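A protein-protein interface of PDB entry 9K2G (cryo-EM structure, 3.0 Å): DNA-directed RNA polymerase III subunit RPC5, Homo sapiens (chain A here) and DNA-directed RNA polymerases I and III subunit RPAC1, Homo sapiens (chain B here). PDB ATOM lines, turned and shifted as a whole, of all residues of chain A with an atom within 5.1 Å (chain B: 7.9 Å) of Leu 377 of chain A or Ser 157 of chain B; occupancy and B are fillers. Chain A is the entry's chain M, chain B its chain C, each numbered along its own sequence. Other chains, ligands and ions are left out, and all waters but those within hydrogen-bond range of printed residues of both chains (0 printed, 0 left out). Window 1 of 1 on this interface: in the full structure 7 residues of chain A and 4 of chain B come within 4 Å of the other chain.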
ATOM      1  N   SER A 342       1.377 -22.228  -2.425  1.00  0.00           N
ATOM      2  CA  SER A 342       2.199 -22.127  -3.624  1.00  0.00           C
ATOM      3  C   SER A 342       1.996 -23.257  -4.621  1.00  0.00           C
ATOM      4  O   SER A 342       2.358 -23.089  -5.789  1.00  0.00           O
ATOM      5  CB  SER A 342       3.689 -22.066  -3.251  1.00  0.00           C
ATOM      6  OG  SER A 342       4.096 -23.253  -2.595  1.00  0.00           O
ATOM      7  N   VAL A 344       3.563 -26.121  -4.691  1.00  0.00           N
ATOM      8  CA  VAL A 344       4.795 -26.877  -4.902  1.00  0.00           C
ATOM      9  C   VAL A 344       4.562 -28.322  -4.491  1.00  0.00           C
ATOM     10  O   VAL A 344       3.697 -28.596  -3.646  1.00  0.00           O
ATOM     11  CB  VAL A 344       5.972 -26.251  -4.131  1.00  0.00           C
ATOM     12  CG1 VAL A 344       6.251 -24.848  -4.638  1.00  0.00           C
ATOM     13  CG2 VAL A 344       5.689 -26.239  -2.640  1.00  0.00           C
ATOM     14  N   VAL A 348       9.170 -31.086  -1.775  1.00  0.00           N
ATOM     15  CA  VAL A 348       9.872 -29.858  -1.402  1.00  0.00           C
ATOM     16  C   VAL A 348       9.440 -29.395  -0.018  1.00  0.00           C
ATOM     17  O   VAL A 348      10.264 -28.930   0.784  1.00  0.00           O
ATOM     18  CB  VAL A 348       9.638 -28.773  -2.464  1.00  0.00           C
ATOM     19  CG1 VAL A 348      10.392 -27.507  -2.089  1.00  0.00           C
ATOM     20  CG2 VAL A 348      10.056 -29.275  -3.839  1.00  0.00           C
ATOM     21  N   GLY A 352      11.894 -28.893   3.183  1.00  0.00           N
ATOM     22  CA  GLY A 352      11.959 -27.651   3.940  1.00  0.00           C
ATOM     23  C   GLY A 352      11.648 -27.844   5.411  1.00  0.00           C
ATOM     24  O   GLY A 352      12.334 -27.293   6.281  1.00  0.00           O
ATOM     25  N   ALA A 372      14.296 -18.939   4.672  1.00  0.00           N
ATOM     26  CA  ALA A 372      13.786 -18.557   3.360  1.00  0.00           C
ATOM     27  C   ALA A 372      14.904 -18.540   2.318  1.00  0.00           C
ATOM     28  O   ALA A 372      14.707 -18.974   1.177  1.00  0.00           O
ATOM     29  CB  ALA A 372      13.101 -17.192   3.431  1.00  0.00           C
ATOM     30  N   THR A 375      16.156 -22.470   1.779  1.00  0.00           N
ATOM     31  CA  THR A 375      15.197 -23.365   1.142  1.00  0.00           C
ATOM     32  C   THR A 375      14.625 -22.808  -0.158  1.00  0.00           C
ATOM     33  O   THR A 375      13.953 -23.553  -0.879  1.00  0.00           O
ATOM     34  CB  THR A 375      14.045 -23.675   2.109  1.00  0.00           C
ATOM     35  OG1 THR A 375      13.320 -22.473   2.392  1.00  0.00           O
ATOM     36  CG2 THR A 375      14.586 -24.257   3.405  1.00  0.00           C
ATOM     37  N   LYS A 376      14.870 -21.535  -0.467  1.00  0.00           N
ATOM     38  CA  LYS A 376      14.357 -20.880  -1.671  1.00  0.00           C
ATOM     39  C   LYS A 376      12.833 -20.912  -1.748  1.00  0.00           C
ATOM     40  O   LYS A 376      12.258 -20.757  -2.831  1.00  0.00           O
ATOM     41  CB  LYS A 376      14.962 -21.493  -2.946  1.00  0.00           C
ATOM     42  CG  LYS A 376      16.483 -21.504  -2.972  1.00  0.00           C
ATOM     43  CD  LYS A 376      17.057 -20.103  -2.836  1.00  0.00           C
ATOM     44  CE  LYS A 376      18.574 -20.127  -2.895  1.00  0.00           C
ATOM     45  NZ  LYS A 376      19.162 -18.799  -2.578  1.00  0.00           N
ATOM     46  N   LEU A 377      12.163 -21.107  -0.618  1.00  0.00           N
ATOM     47  CA  LEU A 377      10.712 -21.203  -0.579  1.00  0.00           C
ATOM     48  C   LEU A 377      10.084 -19.835  -0.334  1.00  0.00           C
ATOM     49  O   LEU A 377      10.750 -18.884   0.079  1.00  0.00           O
ATOM     50  CB  LEU A 377      10.267 -22.188   0.502  1.00  0.00           C
ATOM     51  CG  LEU A 377      10.463 -23.677   0.191  1.00  0.00           C
ATOM     52  CD1 LEU A 377      10.238 -24.519   1.434  1.00  0.00           C
ATOM     53  CD2 LEU A 377       9.531 -24.106  -0.927  1.00  0.00           C
ATOM     54  N   CYS A 378       8.784 -19.752  -0.597  1.00  0.00           N
ATOM     55  CA  CYS A 378       8.057 -18.509  -0.391  1.00  0.00           C
ATOM     56  C   CYS A 378       7.888 -18.232   1.102  1.00  0.00           C
ATOM     57  O   CYS A 378       8.054 -19.113   1.952  1.00  0.00           O
ATOM     58  CB  CYS A 378       6.698 -18.555  -1.081  1.00  0.00           C
ATOM     59  SG  CYS A 378       5.532 -19.730  -0.362  1.00  0.00           S
ATOM     60  N   ALA A 379       7.544 -16.981   1.412  1.00  0.00           N
ATOM     61  CA  ALA A 379       7.462 -16.550   2.806  1.00  0.00           C
ATOM     62  C   ALA A 379       6.356 -17.283   3.563  1.00  0.00           C
ATOM     63  O   ALA A 379       6.553 -17.691   4.712  1.00  0.00           O
ATOM     64  CB  ALA A 379       7.242 -15.042   2.873  1.00  0.00           C
ATOM     65  N   ASP A 381       4.966 -20.253   3.077  1.00  0.00           N
ATOM     66  CA  ASP A 381       5.282 -21.650   3.376  1.00  0.00           C
ATOM     67  C   ASP A 381       6.233 -21.757   4.565  1.00  0.00           C
ATOM     68  O   ASP A 381       6.063 -22.630   5.429  1.00  0.00           O
ATOM     69  CB  ASP A 381       5.874 -22.336   2.146  1.00  0.00           C
ATOM     70  CG  ASP A 381       4.810 -22.761   1.154  1.00  0.00           C
ATOM     71  OD1 ASP A 381       3.668 -23.029   1.585  1.00  0.00           O
ATOM     72  OD2 ASP A 381       5.114 -22.832  -0.054  1.00  0.00           O
ATOM     73  N   VAL A 382       7.239 -20.882   4.633  1.00  0.00           N
ATOM     74  CA  VAL A 382       8.141 -20.865   5.781  1.00  0.00           C
ATOM     75  C   VAL A 382       7.377 -20.499   7.051  1.00  0.00           C
ATOM     76  O   VAL A 382       7.627 -21.055   8.129  1.00  0.00           O
ATOM     77  CB  VAL A 382       9.317 -19.902   5.523  1.00  0.00           C
ATOM     78  CG1 VAL A 382      10.234 -19.835   6.737  1.00  0.00           C
ATOM     79  CG2 VAL A 382      10.097 -20.336   4.287  1.00  0.00           C
ATOM     80  N   PHE A 385       5.556 -23.525   8.153  1.00  0.00           N
ATOM     81  CA  PHE A 385       6.489 -24.460   8.779  1.00  0.00           C
ATOM     82  C   PHE A 385       6.807 -24.045  10.206  1.00  0.00           C
ATOM     83  O   PHE A 385       6.828 -24.878  11.121  1.00  0.00           O
ATOM     84  CB  PHE A 385       7.776 -24.546   7.952  1.00  0.00           C
ATOM     85  CG  PHE A 385       7.610 -25.213   6.620  1.00  0.00           C
ATOM     86  CD1 PHE A 385       6.546 -26.070   6.381  1.00  0.00           C
ATOM     87  CD2 PHE A 385       8.523 -24.984   5.605  1.00  0.00           C
ATOM     88  CE1 PHE A 385       6.404 -26.683   5.153  1.00  0.00           C
ATOM     89  CE2 PHE A 385       8.381 -25.595   4.375  1.00  0.00           C
ATOM     90  CZ  PHE A 385       7.321 -26.444   4.148  1.00  0.00           C
ATOM     91  N   ALA B 153      15.874 -23.320  -9.888  1.00  0.00           N
ATOM     92  CA  ALA B 153      15.788 -24.551  -9.126  1.00  0.00           C
ATOM     93  C   ALA B 153      14.506 -25.304  -9.471  1.00  0.00           C
ATOM     94  O   ALA B 153      13.574 -24.761 -10.074  1.00  0.00           O
ATOM     95  CB  ALA B 153      15.851 -24.254  -7.626  1.00  0.00           C
ATOM     96  N   LYS B 154      14.471 -26.578  -9.084  1.00  0.00           N
ATOM     97  CA  LYS B 154      13.316 -27.416  -9.398  1.00  0.00           C
ATOM     98  C   LYS B 154      12.057 -26.895  -8.713  1.00  0.00           C
ATOM     99  O   LYS B 154      10.981 -26.865  -9.323  1.00  0.00           O
ATOM    100  CB  LYS B 154      13.590 -28.860  -8.989  1.00  0.00           C
ATOM    101  CG  LYS B 154      14.963 -29.366  -9.409  1.00  0.00           C
ATOM    102  CD  LYS B 154      15.193 -29.179 -10.900  1.00  0.00           C
ATOM    103  CE  LYS B 154      16.681 -29.130 -11.216  1.00  0.00           C
ATOM    104  NZ  LYS B 154      17.356 -28.031 -10.467  1.00  0.00           N
ATOM    105  N   ASP B 155      12.170 -26.483  -7.452  1.00  0.00           N
ATOM    106  CA  ASP B 155      11.014 -25.949  -6.733  1.00  0.00           C
ATOM    107  C   ASP B 155      10.795 -24.474  -7.067  1.00  0.00           C
ATOM    108  O   ASP B 155       9.788 -24.109  -7.680  1.00  0.00           O
ATOM    109  CB  ASP B 155      11.192 -26.153  -5.228  1.00  0.00           C
ATOM    110  CG  ASP B 155      12.582 -25.770  -4.744  1.00  0.00           C
ATOM    111  OD1 ASP B 155      13.423 -25.397  -5.590  1.00  0.00           O
ATOM    112  OD2 ASP B 155      12.834 -25.833  -3.521  1.00  0.00           O
ATOM    113  N   SER B 156      11.750 -23.624  -6.692  1.00  0.00           N
ATOM    114  CA  SER B 156      11.709 -22.185  -6.937  1.00  0.00           C
ATOM    115  C   SER B 156      10.347 -21.593  -6.574  1.00  0.00           C
ATOM    116  O   SER B 156       9.626 -21.053  -7.409  1.00  0.00           O
ATOM    117  CB  SER B 156      12.076 -21.875  -8.391  1.00  0.00           C
ATOM    118  OG  SER B 156      13.385 -22.320  -8.695  1.00  0.00           O
ATOM    119  N   SER B 157       9.994 -21.719  -5.293  1.00  0.00           N
ATOM    120  CA  SER B 157       8.708 -21.199  -4.835  1.00  0.00           C
ATOM    121  C   SER B 157       8.643 -19.680  -4.961  1.00  0.00           C
ATOM    122  O   SER B 157       7.606 -19.125  -5.329  1.00  0.00           O
ATOM    123  CB  SER B 157       8.442 -21.634  -3.396  1.00  0.00           C
ATOM    124  OG  SER B 157       7.126 -21.286  -2.995  1.00  0.00           O
ATOM    125  N   ASP B 158       9.744 -18.998  -4.655  1.00  0.00           N
ATOM    126  CA  ASP B 158       9.760 -17.547  -4.749  1.00  0.00           C
ATOM    127  C   ASP B 158       9.679 -17.111  -6.213  1.00  0.00           C
ATOM    128  O   ASP B 158      10.352 -17.689  -7.075  1.00  0.00           O
ATOM    129  CB  ASP B 158      11.021 -16.973  -4.104  1.00  0.00           C
ATOM    130  CG  ASP B 158      12.290 -17.380  -4.824  1.00  0.00           C
ATOM    131  OD1 ASP B 158      12.412 -18.569  -5.197  1.00  0.00           O
ATOM    132  OD2 ASP B 158      13.166 -16.515  -5.028  1.00  0.00           O
ATOM    133  N   PRO B 159       8.857 -16.109  -6.533  1.00  0.00           N
ATOM    134  CA  PRO B 159       8.790 -15.619  -7.921  1.00  0.00           C
ATOM    135  C   PRO B 159      10.091 -15.014  -8.418  1.00  0.00           C
ATOM    136  O   PRO B 159      10.289 -14.934  -9.638  1.00  0.00           O
ATOM    137  CB  PRO B 159       7.668 -14.575  -7.872  1.00  0.00           C
ATOM    138  CG  PRO B 159       6.877 -14.911  -6.644  1.00  0.00           C
ATOM    139  CD  PRO B 159       7.873 -15.444  -5.663  1.00  0.00           C
ATOM    140  N   ASN B 160      10.975 -14.569  -7.521  1.00  0.00           N
ATOM    141  CA  ASN B 160      12.222 -13.945  -7.952  1.00  0.00           C
ATOM    142  C   ASN B 160      13.095 -14.924  -8.728  1.00  0.00           C
ATOM    143  O   ASN B 160      13.689 -14.566  -9.751  1.00  0.00           O
ATOM    144  CB  ASN B 160      12.977 -13.392  -6.746  1.00  0.00           C
ATOM    145  CG  ASN B 160      12.230 -12.264  -6.059  1.00  0.00           C
ATOM    146  OD1 ASN B 160      11.803 -12.397  -4.914  1.00  0.00           O
ATOM    147  ND2 ASN B 160      12.074 -11.145  -6.756  1.00  0.00           N
ATOM    148  N   GLU B 161      13.189 -16.169  -8.254  1.00  0.00           N
ATOM    149  CA  GLU B 161      14.008 -17.163  -8.941  1.00  0.00           C
ATOM    150  C   GLU B 161      13.335 -17.664 -10.214  1.00  0.00           C
ATOM    151  O   GLU B 161      14.005 -17.871 -11.232  1.00  0.00           O
ATOM    152  CB  GLU B 161      14.309 -18.329  -8.002  1.00  0.00           C
ATOM    153  CG  GLU B 161      15.335 -19.315  -8.535  1.00  0.00           C
ATOM    154  CD  GLU B 161      15.615 -20.445  -7.564  1.00  0.00           C
ATOM    155  OE1 GLU B 161      14.730 -20.757  -6.739  1.00  0.00           O
ATOM    156  OE2 GLU B 161      16.723 -21.022  -7.625  1.00  0.00           O
ATOM    157  N   LEU B 162      12.013 -17.860 -10.175  1.00  0.00           N
ATOM    158  CA  LEU B 162      11.299 -18.379 -11.339  1.00  0.00           C
ATOM    159  C   LEU B 162      11.297 -17.383 -12.492  1.00  0.00           C
ATOM    160  O   LEU B 162      11.468 -17.774 -13.654  1.00  0.00           O
ATOM    161  CB  LEU B 162       9.861 -18.732 -10.962  1.00  0.00           C
ATOM    162  CG  LEU B 162       9.561 -20.119 -10.405  1.00  0.00           C
ATOM    163  CD1 LEU B 162       8.079 -20.243 -10.085  1.00  0.00           C
ATOM    164  CD2 LEU B 162       9.992 -21.211 -11.375  1.00  0.00           C
ATOM    165  N   TYR B 163      11.101 -16.105 -12.200  1.00  0.00           N
ATOM    166  CA  TYR B 163      10.770 -15.121 -13.216  1.00  0.00           C
ATOM    167  C   TYR B 163      11.803 -14.004 -13.263  1.00  0.00           C
ATOM    168  O   TYR B 163      12.527 -13.749 -12.294  1.00  0.00           O
ATOM    169  CB  TYR B 163       9.376 -14.525 -12.968  1.00  0.00           C
ATOM    170  CG  TYR B 163       8.318 -15.570 -12.673  1.00  0.00           C
ATOM    171  CD1 TYR B 163       7.864 -16.422 -13.665  1.00  0.00           C
ATOM    172  CD2 TYR B 163       7.776 -15.697 -11.399  1.00  0.00           C
ATOM    173  CE1 TYR B 163       6.901 -17.380 -13.401  1.00  0.00           C
ATOM    174  CE2 TYR B 163       6.810 -16.653 -11.126  1.00  0.00           C
ATOM    175  CZ  TYR B 163       6.377 -17.489 -12.134  1.00  0.00           C
ATOM    176  OH  TYR B 163       5.413 -18.440 -11.872  1.00  0.00           O
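Printed residues of chain B within 4 Å of Lys 376 of chain A: Ser 157, Asp 158 and Glu 161.
Of chain B, only Ser 157 (3.6 Å) comes within 4 Å of Leu 377 of chain A.
Of chain B, only Ser 157 comes within 4 Å of Cys 378 of chain A.
Of the printed residues of chain B, Asp 381 of chain A touches Ser 157.
Of the printed residues of chain A, Asp 155 of chain B touches Val 348 and Thr 375.
Printed residues of chain A within 4 Å of Asp 158 of chain B: Lys 376 (3.2 Å).
The nearest residue of chain B that does not touch Leu 377 of chain A is Asp 158 of chain B (4.4 Å).
Hydrophobic or aromatic side chains of chain A within 4 Å of the printed part of chain B: Val 348 and Leu 377.
Printed residues of chain B that touch a printed residue of chain A: Asp 155, Ser 157, Asp 158 and Glu 161.
CB of Ser 342 of chain A touches OG of Ser 157 of chain B (3.5 Å).
CG1 of Val 348 of chain A touches OD2 of Asp 155 of chain B, at 3.3 Å.
Thr 375 of chain A touches Asp 155 of chain B.
OE1 of Glu 161 of chain B touches CB of Lys 376 of chain A, at 3.9 Å.
Leu 377 of chain A touches Ser 157 of chain B (CA to CB, 3.6 Å).
Asp 381 of chain A touches Ser 157 of chain B (OD2 to OG, 3.9 Å).
N of Cys 378 of chain A sits at hydrogen-bond distance from OG of Ser 157 of chain B, at 3.3 Å.
The backbone carbonyl oxygen (O) of Lys 376 of chain A is in hydrogen-bond range of the backbone NH (N) of Ser 157 of chain B (3.5 Å).
O of Lys 376 of chain A lies close to OD1 of Asp 158 of chain B, 3.2 Å away.
SG of Cys 378 of chain A sits at hydrogen-bond distance from OD2 of Asp 381 of chain A, 3.1 Å away.
The backbone NH (N) of Ala 153 of chain B is in hydrogen-bond range of the side-chain carboxylate (OE2) of Glu 161 of chain B.
The side-chain carboxylate (OD2) of Asp 381 of chain A is in hydrogen-bond range of the side-chain hydroxyl (OG) of Ser 342 of chain A (2.8 Å).
The backbone NH (N) of Glu 161 of chain B sits at hydrogen-bond distance from the side-chain carboxylate (OD2) of Asp 158 of chain B.
OE1 of Glu 161 of chain B lies within hydrogen-bond range of OG of Ser 156 of chain B (2.8 Å).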
